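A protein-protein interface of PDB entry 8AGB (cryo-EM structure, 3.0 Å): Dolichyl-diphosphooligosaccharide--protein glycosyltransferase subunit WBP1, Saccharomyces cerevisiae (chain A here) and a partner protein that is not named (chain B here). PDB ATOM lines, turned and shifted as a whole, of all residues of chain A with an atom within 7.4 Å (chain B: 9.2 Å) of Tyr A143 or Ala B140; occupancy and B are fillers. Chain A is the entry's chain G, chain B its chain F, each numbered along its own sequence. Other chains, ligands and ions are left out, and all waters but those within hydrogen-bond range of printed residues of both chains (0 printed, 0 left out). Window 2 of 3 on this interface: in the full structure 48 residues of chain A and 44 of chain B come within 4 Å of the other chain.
The backbone NH of Phe B79 sits at hydrogen-bond distance from the backbone carbonyl oxygen of Ala B140, 3.0 Å away. The backbone carbonyl oxygen of Ala B140 is in hydrogen-bond range of the backbone NH of Gln B80, 2.8 Å away. The backbone carbonyl oxygen (O) of Thr B82 lies within hydrogen-bond range of the backbone NH (N) of Ile B138 (3.1 Å). The backbone carbonyl oxygen (O) of Phe A199 is in hydrogen-bond range of the backbone NH (N) of Arg A141, at 2.9 Å. OG1 of Thr A197 is in hydrogen-bond range of OD1 of Asp A142, at 3.0 Å.
The side-chain hydroxyl of Ser B142 sits close to the side-chain hydroxyl of Tyr A143, 2.3 Å away.
Among the printed residues, pairs that only touch across the chains: Tyr A143 with Phe B79 (3.3 Å), Tyr A143 with Gln B80 (3.2 Å), Tyr A143 with Ala B140 (3.6 Å), Phe A144 with Ile B138 (3.9 Å), Phe A144 with Asn B149 (3.4 Å), Thr A197 with Gln B80 (3.7 Å), Thr A197 with Ile B138 (3.8 Å), Thr A197 with Phe B151 (3.8 Å), Phe A199 with Phe B79 (3.6 Å), Phe A199 with Gln B80 (3.4 Å) and Glu A201 with Phe B79 (3.2 Å).
Printed residues of chain A that touch a printed residue of chain B: Tyr A143, Phe A144, Thr A197, Phe A199 and Glu A201. Hydrophobic or aromatic side chains of chain A that line the printed part of chain B: Tyr A143, Phe A144 and Phe A199. Hydrophobic or aromatic side chains of chain B within 4 Å of the printed part of chain A: Phe B79, Ile B138, Ala B140 and Phe B151.
No residue of chain B comes within 4 Å of Asp A142. Tyr A143 touches four residues of chain B. Printed residues of chain B within 4 Å of Phe A144: Ile B138 (3.9 Å) and Asn B149 (3.4 Å). Printed residues of chain A within 4 Å of Ile B138: Phe A144 (3.9 Å) and Thr A197 (3.8 Å). Ala B140 touches just one residue of chain A: Tyr A143 (3.6 Å). Of the printed residues of chain A, Ser B142 touches Tyr A143. The nearest residue of chain A that does not touch Ala B140 is Phe A144 (4.2 Å).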
ATOM      1  N   ARG A 141      26.614 -26.373   4.202  1.00  0.00           N
ATOM      2  CA  ARG A 141      25.826 -26.786   3.056  1.00  0.00           C
ATOM      3  C   ARG A 141      24.594 -25.898   3.059  1.00  0.00           C
ATOM      4  O   ARG A 141      24.055 -25.579   4.124  1.00  0.00           O
ATOM      5  CB  ARG A 141      25.434 -28.261   3.144  1.00  0.00           C
ATOM      6  CG  ARG A 141      25.955 -29.109   2.001  1.00  0.00           C
ATOM      7  CD  ARG A 141      27.348 -29.626   2.310  1.00  0.00           C
ATOM      8  NE  ARG A 141      28.322 -29.232   1.296  1.00  0.00           N
ATOM      9  CZ  ARG A 141      28.943 -30.084   0.487  1.00  0.00           C
ATOM     10  NH1 ARG A 141      29.814 -29.638  -0.407  1.00  0.00           N
ATOM     11  NH2 ARG A 141      28.695 -31.385   0.574  1.00  0.00           N
ATOM     12  N   ASP A 142      24.138 -25.499   1.873  1.00  0.00           N
ATOM     13  CA  ASP A 142      23.045 -24.532   1.816  1.00  0.00           C
ATOM     14  C   ASP A 142      22.302 -24.651   0.490  1.00  0.00           C
ATOM     15  O   ASP A 142      22.793 -24.181  -0.540  1.00  0.00           O
ATOM     16  CB  ASP A 142      23.570 -23.121   2.012  1.00  0.00           C
ATOM     17  CG  ASP A 142      22.534 -22.066   1.692  1.00  0.00           C
ATOM     18  OD1 ASP A 142      21.352 -22.267   2.039  1.00  0.00           O
ATOM     19  OD2 ASP A 142      22.896 -21.045   1.073  1.00  0.00           O
ATOM     20  N   TYR A 143      21.132 -25.276   0.527  1.00  0.00           N
ATOM     21  CA  TYR A 143      20.299 -25.389  -0.659  1.00  0.00           C
ATOM     22  C   TYR A 143      19.584 -24.049  -0.818  1.00  0.00           C
ATOM     23  O   TYR A 143      19.889 -23.083  -0.114  1.00  0.00           O
ATOM     24  CB  TYR A 143      19.364 -26.584  -0.531  1.00  0.00           C
ATOM     25  CG  TYR A 143      20.038 -27.763   0.126  1.00  0.00           C
ATOM     26  CD1 TYR A 143      21.214 -28.287  -0.391  1.00  0.00           C
ATOM     27  CD2 TYR A 143      19.517 -28.334   1.276  1.00  0.00           C
ATOM     28  CE1 TYR A 143      21.847 -29.352   0.211  1.00  0.00           C
ATOM     29  CE2 TYR A 143      20.141 -29.404   1.883  1.00  0.00           C
ATOM     30  CZ  TYR A 143      21.307 -29.905   1.349  1.00  0.00           C
ATOM     31  OH  TYR A 143      21.931 -30.977   1.947  1.00  0.00           O
ATOM     32  N   PHE A 144      18.618 -23.964  -1.732  1.00  0.00           N
ATOM     33  CA  PHE A 144      17.942 -22.696  -2.018  1.00  0.00           C
ATOM     34  C   PHE A 144      18.972 -21.627  -2.376  1.00  0.00           C
ATOM     35  O   PHE A 144      18.828 -20.453  -2.031  1.00  0.00           O
ATOM     36  CB  PHE A 144      17.097 -22.213  -0.836  1.00  0.00           C
ATOM     37  CG  PHE A 144      16.215 -23.260  -0.233  1.00  0.00           C
ATOM     38  CD1 PHE A 144      14.952 -23.498  -0.735  1.00  0.00           C
ATOM     39  CD2 PHE A 144      16.638 -23.974   0.873  1.00  0.00           C
ATOM     40  CE1 PHE A 144      14.139 -24.450  -0.160  1.00  0.00           C
ATOM     41  CE2 PHE A 144      15.830 -24.926   1.451  1.00  0.00           C
ATOM     42  CZ  PHE A 144      14.579 -25.163   0.936  1.00  0.00           C
ATOM     43  N   SER A 145      20.023 -22.039  -3.073  1.00  0.00           N
ATOM     44  CA  SER A 145      21.086 -21.107  -3.395  1.00  0.00           C
ATOM     45  C   SER A 145      21.140 -20.832  -4.893  1.00  0.00           C
ATOM     46  O   SER A 145      20.706 -21.662  -5.699  1.00  0.00           O
ATOM     47  CB  SER A 145      22.440 -21.655  -2.929  1.00  0.00           C
ATOM     48  OG  SER A 145      23.463 -21.378  -3.869  1.00  0.00           O
ATOM     49  N   PRO A 146      21.648 -19.660  -5.291  1.00  0.00           N
ATOM     50  CA  PRO A 146      21.631 -19.304  -6.719  1.00  0.00           C
ATOM     51  C   PRO A 146      22.317 -20.324  -7.608  1.00  0.00           C
ATOM     52  O   PRO A 146      21.813 -20.624  -8.697  1.00  0.00           O
ATOM     53  CB  PRO A 146      22.360 -17.956  -6.731  1.00  0.00           C
ATOM     54  CG  PRO A 146      21.973 -17.347  -5.428  1.00  0.00           C
ATOM     55  CD  PRO A 146      21.985 -18.498  -4.447  1.00  0.00           C
ATOM     56  N   LEU A 151      29.033 -21.949  -2.662  1.00  0.00           N
ATOM     57  CA  LEU A 151      28.218 -21.192  -1.716  1.00  0.00           C
ATOM     58  C   LEU A 151      28.241 -19.716  -2.101  1.00  0.00           C
ATOM     59  O   LEU A 151      29.075 -18.926  -1.649  1.00  0.00           O
ATOM     60  CB  LEU A 151      28.699 -21.407  -0.288  1.00  0.00           C
ATOM     61  CG  LEU A 151      27.862 -20.661   0.751  1.00  0.00           C
ATOM     62  CD1 LEU A 151      26.494 -21.296   0.879  1.00  0.00           C
ATOM     63  CD2 LEU A 151      28.561 -20.629   2.091  1.00  0.00           C
ATOM     64  N   PRO A 195      23.276 -17.944   5.073  1.00  0.00           N
ATOM     65  CA  PRO A 195      21.884 -17.982   4.617  1.00  0.00           C
ATOM     66  C   PRO A 195      21.005 -18.694   5.632  1.00  0.00           C
ATOM     67  O   PRO A 195      21.442 -19.616   6.323  1.00  0.00           O
ATOM     68  CB  PRO A 195      21.969 -18.755   3.299  1.00  0.00           C
ATOM     69  CG  PRO A 195      23.338 -18.439   2.808  1.00  0.00           C
ATOM     70  CD  PRO A 195      24.187 -18.474   4.046  1.00  0.00           C
ATOM     71  N   THR A 197      18.861 -20.851   5.467  1.00  0.00           N
ATOM     72  CA  THR A 197      18.625 -22.268   5.232  1.00  0.00           C
ATOM     73  C   THR A 197      19.917 -23.077   5.185  1.00  0.00           C
ATOM     74  O   THR A 197      19.941 -24.162   4.596  1.00  0.00           O
ATOM     75  CB  THR A 197      17.843 -22.465   3.934  1.00  0.00           C
ATOM     76  OG1 THR A 197      18.511 -21.782   2.868  1.00  0.00           O
ATOM     77  CG2 THR A 197      16.438 -21.910   4.075  1.00  0.00           C
ATOM     78  N   SER A 198      20.994 -22.575   5.784  1.00  0.00           N
ATOM     79  CA  SER A 198      22.302 -23.209   5.701  1.00  0.00           C
ATOM     80  C   SER A 198      22.651 -23.903   7.011  1.00  0.00           C
ATOM     81  O   SER A 198      22.365 -23.386   8.094  1.00  0.00           O
ATOM     82  CB  SER A 198      23.381 -22.177   5.378  1.00  0.00           C
ATOM     83  OG  SER A 198      23.655 -21.377   6.511  1.00  0.00           O
ATOM     84  N   PHE A 199      23.276 -25.074   6.901  1.00  0.00           N
ATOM     85  CA  PHE A 199      23.598 -25.894   8.060  1.00  0.00           C
ATOM     86  C   PHE A 199      24.963 -26.539   7.866  1.00  0.00           C
ATOM     87  O   PHE A 199      25.377 -26.816   6.741  1.00  0.00           O
ATOM     88  CB  PHE A 199      22.516 -26.955   8.316  1.00  0.00           C
ATOM     89  CG  PHE A 199      22.412 -27.996   7.240  1.00  0.00           C
ATOM     90  CD1 PHE A 199      21.613 -27.784   6.133  1.00  0.00           C
ATOM     91  CD2 PHE A 199      23.091 -29.196   7.348  1.00  0.00           C
ATOM     92  CE1 PHE A 199      21.505 -28.739   5.147  1.00  0.00           C
ATOM     93  CE2 PHE A 199      22.986 -30.155   6.364  1.00  0.00           C
ATOM     94  CZ  PHE A 199      22.193 -29.926   5.261  1.00  0.00           C
ATOM     95  N   GLU A 201      27.101 -29.567   7.821  1.00  0.00           N
ATOM     96  CA  GLU A 201      26.892 -31.004   7.645  1.00  0.00           C
ATOM     97  C   GLU A 201      28.189 -31.752   7.937  1.00  0.00           C
ATOM     98  O   GLU A 201      29.101 -31.788   7.107  1.00  0.00           O
ATOM     99  CB  GLU A 201      26.399 -31.305   6.235  1.00  0.00           C
ATOM    100  CG  GLU A 201      25.944 -32.739   6.037  1.00  0.00           C
ATOM    101  CD  GLU A 201      25.483 -33.011   4.620  1.00  0.00           C
ATOM    102  OE1 GLU A 201      25.506 -32.074   3.795  1.00  0.00           O
ATOM    103  OE2 GLU A 201      25.098 -34.164   4.331  1.00  0.00           O
ATOM    104  N   SER B  74       3.559 -30.874   1.798  1.00  0.00           N
ATOM    105  CA  SER B  74       4.030 -31.745   0.730  1.00  0.00           C
ATOM    106  C   SER B  74       5.524 -32.031   0.899  1.00  0.00           C
ATOM    107  O   SER B  74       6.107 -31.777   1.957  1.00  0.00           O
ATOM    108  CB  SER B  74       3.722 -31.122  -0.628  1.00  0.00           C
ATOM    109  OG  SER B  74       4.610 -31.600  -1.623  1.00  0.00           O
ATOM    110  N   THR B  75       6.139 -32.607  -0.143  1.00  0.00           N
ATOM    111  CA  THR B  75       7.555 -33.018  -0.179  1.00  0.00           C
ATOM    112  C   THR B  75       7.975 -33.729   1.107  1.00  0.00           C
ATOM    113  O   THR B  75       8.996 -33.420   1.724  1.00  0.00           O
ATOM    114  CB  THR B  75       8.503 -31.850  -0.520  1.00  0.00           C
ATOM    115  OG1 THR B  75       9.859 -32.314  -0.482  1.00  0.00           O
ATOM    116  CG2 THR B  75       8.373 -30.654   0.419  1.00  0.00           C
ATOM    117  N   ASN B  76       7.172 -34.718   1.499  1.00  0.00           N
ATOM    118  CA  ASN B  76       7.358 -35.399   2.775  1.00  0.00           C
ATOM    119  C   ASN B  76       8.404 -36.508   2.725  1.00  0.00           C
ATOM    120  O   ASN B  76       8.113 -37.655   3.083  1.00  0.00           O
ATOM    121  CB  ASN B  76       6.031 -35.989   3.250  1.00  0.00           C
ATOM    122  CG  ASN B  76       4.894 -34.999   3.174  1.00  0.00           C
ATOM    123  OD1 ASN B  76       4.497 -34.583   2.087  1.00  0.00           O
ATOM    124  ND2 ASN B  76       4.365 -34.611   4.327  1.00  0.00           N
ATOM    125  N   LYS B  77       9.617 -36.183   2.288  1.00  0.00           N
ATOM    126  CA  LYS B  77      10.723 -37.133   2.325  1.00  0.00           C
ATOM    127  C   LYS B  77      12.043 -36.368   2.299  1.00  0.00           C
ATOM    128  O   LYS B  77      12.827 -36.503   1.350  1.00  0.00           O
ATOM    129  CB  LYS B  77      10.631 -38.116   1.156  1.00  0.00           C
ATOM    130  CG  LYS B  77      11.508 -39.349   1.298  1.00  0.00           C
ATOM    131  CD  LYS B  77      11.837 -39.968  -0.054  1.00  0.00           C
ATOM    132  CE  LYS B  77      10.592 -40.166  -0.910  1.00  0.00           C
ATOM    133  NZ  LYS B  77      10.366 -39.051  -1.874  1.00  0.00           N
ATOM    134  N   PRO B  78      12.319 -35.548   3.317  1.00  0.00           N
ATOM    135  CA  PRO B  78      13.508 -34.693   3.280  1.00  0.00           C
ATOM    136  C   PRO B  78      14.687 -35.182   4.107  1.00  0.00           C
ATOM    137  O   PRO B  78      14.518 -35.897   5.100  1.00  0.00           O
ATOM    138  CB  PRO B  78      12.950 -33.386   3.826  1.00  0.00           C
ATOM    139  CG  PRO B  78      12.072 -33.882   4.978  1.00  0.00           C
ATOM    140  CD  PRO B  78      11.548 -35.273   4.545  1.00  0.00           C
ATOM    141  N   PHE B  79      15.895 -34.807   3.693  1.00  0.00           N
ATOM    142  CA  PHE B  79      17.092 -35.174   4.436  1.00  0.00           C
ATOM    143  C   PHE B  79      17.369 -34.178   5.557  1.00  0.00           C
ATOM    144  O   PHE B  79      17.714 -34.580   6.673  1.00  0.00           O
ATOM    145  CB  PHE B  79      18.295 -35.260   3.490  1.00  0.00           C
ATOM    146  CG  PHE B  79      19.595 -34.831   4.111  1.00  0.00           C
ATOM    147  CD1 PHE B  79      20.189 -35.585   5.109  1.00  0.00           C
ATOM    148  CD2 PHE B  79      20.217 -33.665   3.701  1.00  0.00           C
ATOM    149  CE1 PHE B  79      21.381 -35.186   5.680  1.00  0.00           C
ATOM    150  CE2 PHE B  79      21.409 -33.263   4.269  1.00  0.00           C
ATOM    151  CZ  PHE B  79      21.991 -34.024   5.260  1.00  0.00           C
ATOM    152  N   GLN B  80      17.217 -32.886   5.276  1.00  0.00           N
ATOM    153  CA  GLN B  80      17.291 -31.832   6.281  1.00  0.00           C
ATOM    154  C   GLN B  80      15.888 -31.350   6.637  1.00  0.00           C
ATOM    155  O   GLN B  80      15.071 -31.083   5.751  1.00  0.00           O
ATOM    156  CB  GLN B  80      18.167 -30.670   5.800  1.00  0.00           C
ATOM    157  CG  GLN B  80      17.481 -29.623   4.928  1.00  0.00           C
ATOM    158  CD  GLN B  80      17.939 -28.209   5.232  1.00  0.00           C
ATOM    159  OE1 GLN B  80      17.784 -27.721   6.351  1.00  0.00           O
ATOM    160  NE2 GLN B  80      18.509 -27.544   4.235  1.00  0.00           N
ATOM    161  N   ASN B  81      15.591 -31.313   7.934  1.00  0.00           N
ATOM    162  CA  ASN B  81      14.264 -30.928   8.405  1.00  0.00           C
ATOM    163  C   ASN B  81      14.405 -30.199   9.732  1.00  0.00           C
ATOM    164  O   ASN B  81      14.875 -30.782  10.713  1.00  0.00           O
ATOM    165  CB  ASN B  81      13.355 -32.150   8.542  1.00  0.00           C
ATOM    166  CG  ASN B  81      14.106 -33.394   8.970  1.00  0.00           C
ATOM    167  OD1 ASN B  81      15.058 -33.327   9.747  1.00  0.00           O
ATOM    168  ND2 ASN B  81      13.681 -34.543   8.459  1.00  0.00           N
ATOM    169  N   THR B  82      14.009 -28.927   9.759  1.00  0.00           N
ATOM    170  CA  THR B  82      14.199 -28.088  10.935  1.00  0.00           C
ATOM    171  C   THR B  82      13.023 -27.129  11.054  1.00  0.00           C
ATOM    172  O   THR B  82      12.310 -26.869  10.082  1.00  0.00           O
ATOM    173  CB  THR B  82      15.519 -27.309  10.856  1.00  0.00           C
ATOM    174  OG1 THR B  82      16.535 -28.140  10.285  1.00  0.00           O
ATOM    175  CG2 THR B  82      15.972 -26.876  12.241  1.00  0.00           C
ATOM    176  N   LEU B 137       9.173 -23.689   8.715  1.00  0.00           N
ATOM    177  CA  LEU B 137       9.570 -25.073   8.517  1.00  0.00           C
ATOM    178  C   LEU B 137      10.361 -25.215   7.222  1.00  0.00           C
ATOM    179  O   LEU B 137      10.019 -24.602   6.206  1.00  0.00           O
ATOM    180  CB  LEU B 137       8.330 -25.970   8.508  1.00  0.00           C
ATOM    181  CG  LEU B 137       8.487 -27.469   8.715  1.00  0.00           C
ATOM    182  CD1 LEU B 137       7.345 -27.996   9.559  1.00  0.00           C
ATOM    183  CD2 LEU B 137       8.478 -28.138   7.375  1.00  0.00           C
ATOM    184  N   ILE B 138      11.417 -26.026   7.261  1.00  0.00           N
ATOM    185  CA  ILE B 138      12.313 -26.234   6.124  1.00  0.00           C
ATOM    186  C   ILE B 138      12.530 -27.725   5.915  1.00  0.00           C
ATOM    187  O   ILE B 138      13.027 -28.413   6.814  1.00  0.00           O
ATOM    188  CB  ILE B 138      13.663 -25.519   6.294  1.00  0.00           C
ATOM    189  CG1 ILE B 138      13.458 -24.027   6.544  1.00  0.00           C
ATOM    190  CG2 ILE B 138      14.534 -25.738   5.071  1.00  0.00           C
ATOM    191  CD1 ILE B 138      14.670 -23.333   7.086  1.00  0.00           C
ATOM    192  N   LEU B 139      12.161 -28.221   4.736  1.00  0.00           N
ATOM    193  CA  LEU B 139      12.484 -29.578   4.315  1.00  0.00           C
ATOM    194  C   LEU B 139      13.192 -29.530   2.970  1.00  0.00           C
ATOM    195  O   LEU B 139      12.747 -28.833   2.054  1.00  0.00           O
ATOM    196  CB  LEU B 139      11.237 -30.458   4.202  1.00  0.00           C
ATOM    197  CG  LEU B 139       9.959 -30.110   4.951  1.00  0.00           C
ATOM    198  CD1 LEU B 139       8.785 -30.008   4.000  1.00  0.00           C
ATOM    199  CD2 LEU B 139       9.696 -31.174   6.002  1.00  0.00           C
ATOM    200  N   ALA B 140      14.293 -30.270   2.860  1.00  0.00           N
ATOM    201  CA  ALA B 140      15.081 -30.321   1.638  1.00  0.00           C
ATOM    202  C   ALA B 140      15.928 -31.585   1.666  1.00  0.00           C
ATOM    203  O   ALA B 140      16.411 -31.986   2.726  1.00  0.00           O
ATOM    204  CB  ALA B 140      15.967 -29.081   1.491  1.00  0.00           C
ATOM    205  N   SER B 141      16.107 -32.200   0.497  1.00  0.00           N
ATOM    206  CA  SER B 141      16.722 -33.520   0.398  1.00  0.00           C
ATOM    207  C   SER B 141      18.057 -33.513  -0.337  1.00  0.00           C
ATOM    208  O   SER B 141      18.586 -34.589  -0.636  1.00  0.00           O
ATOM    209  CB  SER B 141      15.761 -34.495  -0.285  1.00  0.00           C
ATOM    210  OG  SER B 141      16.382 -35.751  -0.501  1.00  0.00           O
ATOM    211  N   SER B 142      18.598 -32.339  -0.660  1.00  0.00           N
ATOM    212  CA  SER B 142      19.913 -32.106  -1.249  1.00  0.00           C
ATOM    213  C   SER B 142      19.960 -32.466  -2.731  1.00  0.00           C
ATOM    214  O   SER B 142      20.949 -32.147  -3.392  1.00  0.00           O
ATOM    215  CB  SER B 142      21.048 -32.865  -0.533  1.00  0.00           C
ATOM    216  OG  SER B 142      20.958 -32.729   0.871  1.00  0.00           O
ATOM    217  N   THR B 143      18.930 -33.112  -3.283  1.00  0.00           N
ATOM    218  CA  THR B 143      18.952 -33.551  -4.674  1.00  0.00           C
ATOM    219  C   THR B 143      17.666 -33.261  -5.427  1.00  0.00           C
ATOM    220  O   THR B 143      17.666 -33.375  -6.656  1.00  0.00           O
ATOM    221  CB  THR B 143      19.235 -35.062  -4.778  1.00  0.00           C
ATOM    222  OG1 THR B 143      18.023 -35.794  -4.552  1.00  0.00           O
ATOM    223  CG2 THR B 143      20.292 -35.512  -3.776  1.00  0.00           C
ATOM    224  N   ALA B 144      16.572 -32.920  -4.748  1.00  0.00           N
ATOM    225  CA  ALA B 144      15.322 -32.629  -5.433  1.00  0.00           C
ATOM    226  C   ALA B 144      15.503 -31.479  -6.418  1.00  0.00           C
ATOM    227  O   ALA B 144      16.370 -30.616  -6.250  1.00  0.00           O
ATOM    228  CB  ALA B 144      14.230 -32.286  -4.419  1.00  0.00           C
ATOM    229  N   LYS B 145      14.679 -31.483  -7.459  1.00  0.00           N
ATOM    230  CA  LYS B 145      14.714 -30.410  -8.440  1.00  0.00           C
ATOM    231  C   LYS B 145      14.436 -29.066  -7.768  1.00  0.00           C
ATOM    232  O   LYS B 145      13.661 -29.002  -6.806  1.00  0.00           O
ATOM    233  CB  LYS B 145      13.713 -30.691  -9.569  1.00  0.00           C
ATOM    234  CG  LYS B 145      12.232 -30.760  -9.177  1.00  0.00           C
ATOM    235  CD  LYS B 145      11.544 -29.403  -9.137  1.00  0.00           C
ATOM    236  CE  LYS B 145      10.092 -29.526  -8.706  1.00  0.00           C
ATOM    237  NZ  LYS B 145       9.461 -28.192  -8.513  1.00  0.00           N
ATOM    238  N   PRO B 146      15.093 -27.993  -8.205  1.00  0.00           N
ATOM    239  CA  PRO B 146      14.856 -26.672  -7.610  1.00  0.00           C
ATOM    240  C   PRO B 146      13.373 -26.333  -7.543  1.00  0.00           C
ATOM    241  O   PRO B 146      12.624 -26.570  -8.494  1.00  0.00           O
ATOM    242  CB  PRO B 146      15.609 -25.725  -8.548  1.00  0.00           C
ATOM    243  CG  PRO B 146      16.689 -26.565  -9.132  1.00  0.00           C
ATOM    244  CD  PRO B 146      16.118 -27.950  -9.262  1.00  0.00           C
ATOM    245  N   LYS B 147      12.957 -25.783  -6.398  1.00  0.00           N
ATOM    246  CA  LYS B 147      11.571 -25.455  -6.024  1.00  0.00           C
ATOM    247  C   LYS B 147      10.789 -26.690  -5.584  1.00  0.00           C
ATOM    248  O   LYS B 147       9.562 -26.628  -5.487  1.00  0.00           O
ATOM    249  CB  LYS B 147      10.827 -24.716  -7.148  1.00  0.00           C
ATOM    250  CG  LYS B 147       9.827 -23.639  -6.699  1.00  0.00           C
ATOM    251  CD  LYS B 147       8.399 -24.146  -6.553  1.00  0.00           C
ATOM    252  CE  LYS B 147       7.406 -22.998  -6.492  1.00  0.00           C
ATOM    253  NZ  LYS B 147       6.014 -23.475  -6.265  1.00  0.00           N
ATOM    254  N   GLU B 148      11.448 -27.816  -5.311  1.00  0.00           N
ATOM    255  CA  GLU B 148      10.755 -28.958  -4.728  1.00  0.00           C
ATOM    256  C   GLU B 148      10.906 -29.002  -3.212  1.00  0.00           C
ATOM    257  O   GLU B 148      10.209 -29.778  -2.551  1.00  0.00           O
ATOM    258  CB  GLU B 148      11.268 -30.269  -5.351  1.00  0.00           C
ATOM    259  CG  GLU B 148      10.613 -31.549  -4.834  1.00  0.00           C
ATOM    260  CD  GLU B 148      10.670 -32.692  -5.827  1.00  0.00           C
ATOM    261  OE1 GLU B 148      10.653 -32.425  -7.044  1.00  0.00           O
ATOM    262  OE2 GLU B 148      10.736 -33.859  -5.388  1.00  0.00           O
ATOM    263  N   ASN B 149      11.745 -28.144  -2.646  1.00  0.00           N
ATOM    264  CA  ASN B 149      11.928 -28.064  -1.209  1.00  0.00           C
ATOM    265  C   ASN B 149      11.010 -26.983  -0.648  1.00  0.00           C
ATOM    266  O   ASN B 149      10.601 -26.058  -1.354  1.00  0.00           O
ATOM    267  CB  ASN B 149      13.387 -27.768  -0.862  1.00  0.00           C
ATOM    268  CG  ASN B 149      14.360 -28.596  -1.674  1.00  0.00           C
ATOM    269  OD1 ASN B 149      15.237 -28.059  -2.350  1.00  0.00           O
ATOM    270  ND2 ASN B 149      14.213 -29.913  -1.610  1.00  0.00           N
ATOM    271  N   LEU B 150      10.687 -27.101   0.636  1.00  0.00           N
ATOM    272  CA  LEU B 150       9.715 -26.222   1.268  1.00  0.00           C
ATOM    273  C   LEU B 150      10.380 -25.329   2.305  1.00  0.00           C
ATOM    274  O   LEU B 150      11.090 -25.817   3.189  1.00  0.00           O
ATOM    275  CB  LEU B 150       8.609 -27.046   1.927  1.00  0.00           C
ATOM    276  CG  LEU B 150       7.286 -26.348   2.225  1.00  0.00           C
ATOM    277  CD1 LEU B 150       6.145 -27.185   1.694  1.00  0.00           C
ATOM    278  CD2 LEU B 150       7.134 -26.118   3.719  1.00  0.00           C
ATOM    279  N   PHE B 151      10.150 -24.009   2.185  1.00  0.00           N
ATOM    280  CA  PHE B 151      10.604 -23.015   3.160  1.00  0.00           C
ATOM    281  C   PHE B 151       9.437 -22.047   3.399  1.00  0.00           C
ATOM    282  O   PHE B 151       9.405 -20.939   2.860  1.00  0.00           O
ATOM    283  CB  PHE B 151      11.857 -22.299   2.651  1.00  0.00           C
ATOM    284  CG  PHE B 151      12.399 -21.250   3.583  1.00  0.00           C
ATOM    285  CD1 PHE B 151      12.152 -21.301   4.944  1.00  0.00           C
ATOM    286  CD2 PHE B 151      13.168 -20.210   3.089  1.00  0.00           C
ATOM    287  CE1 PHE B 151      12.661 -20.335   5.790  1.00  0.00           C
ATOM    288  CE2 PHE B 151      13.674 -19.242   3.931  1.00  0.00           C
ATOM    289  CZ  PHE B 151      13.418 -19.304   5.282  1.00  0.00           C
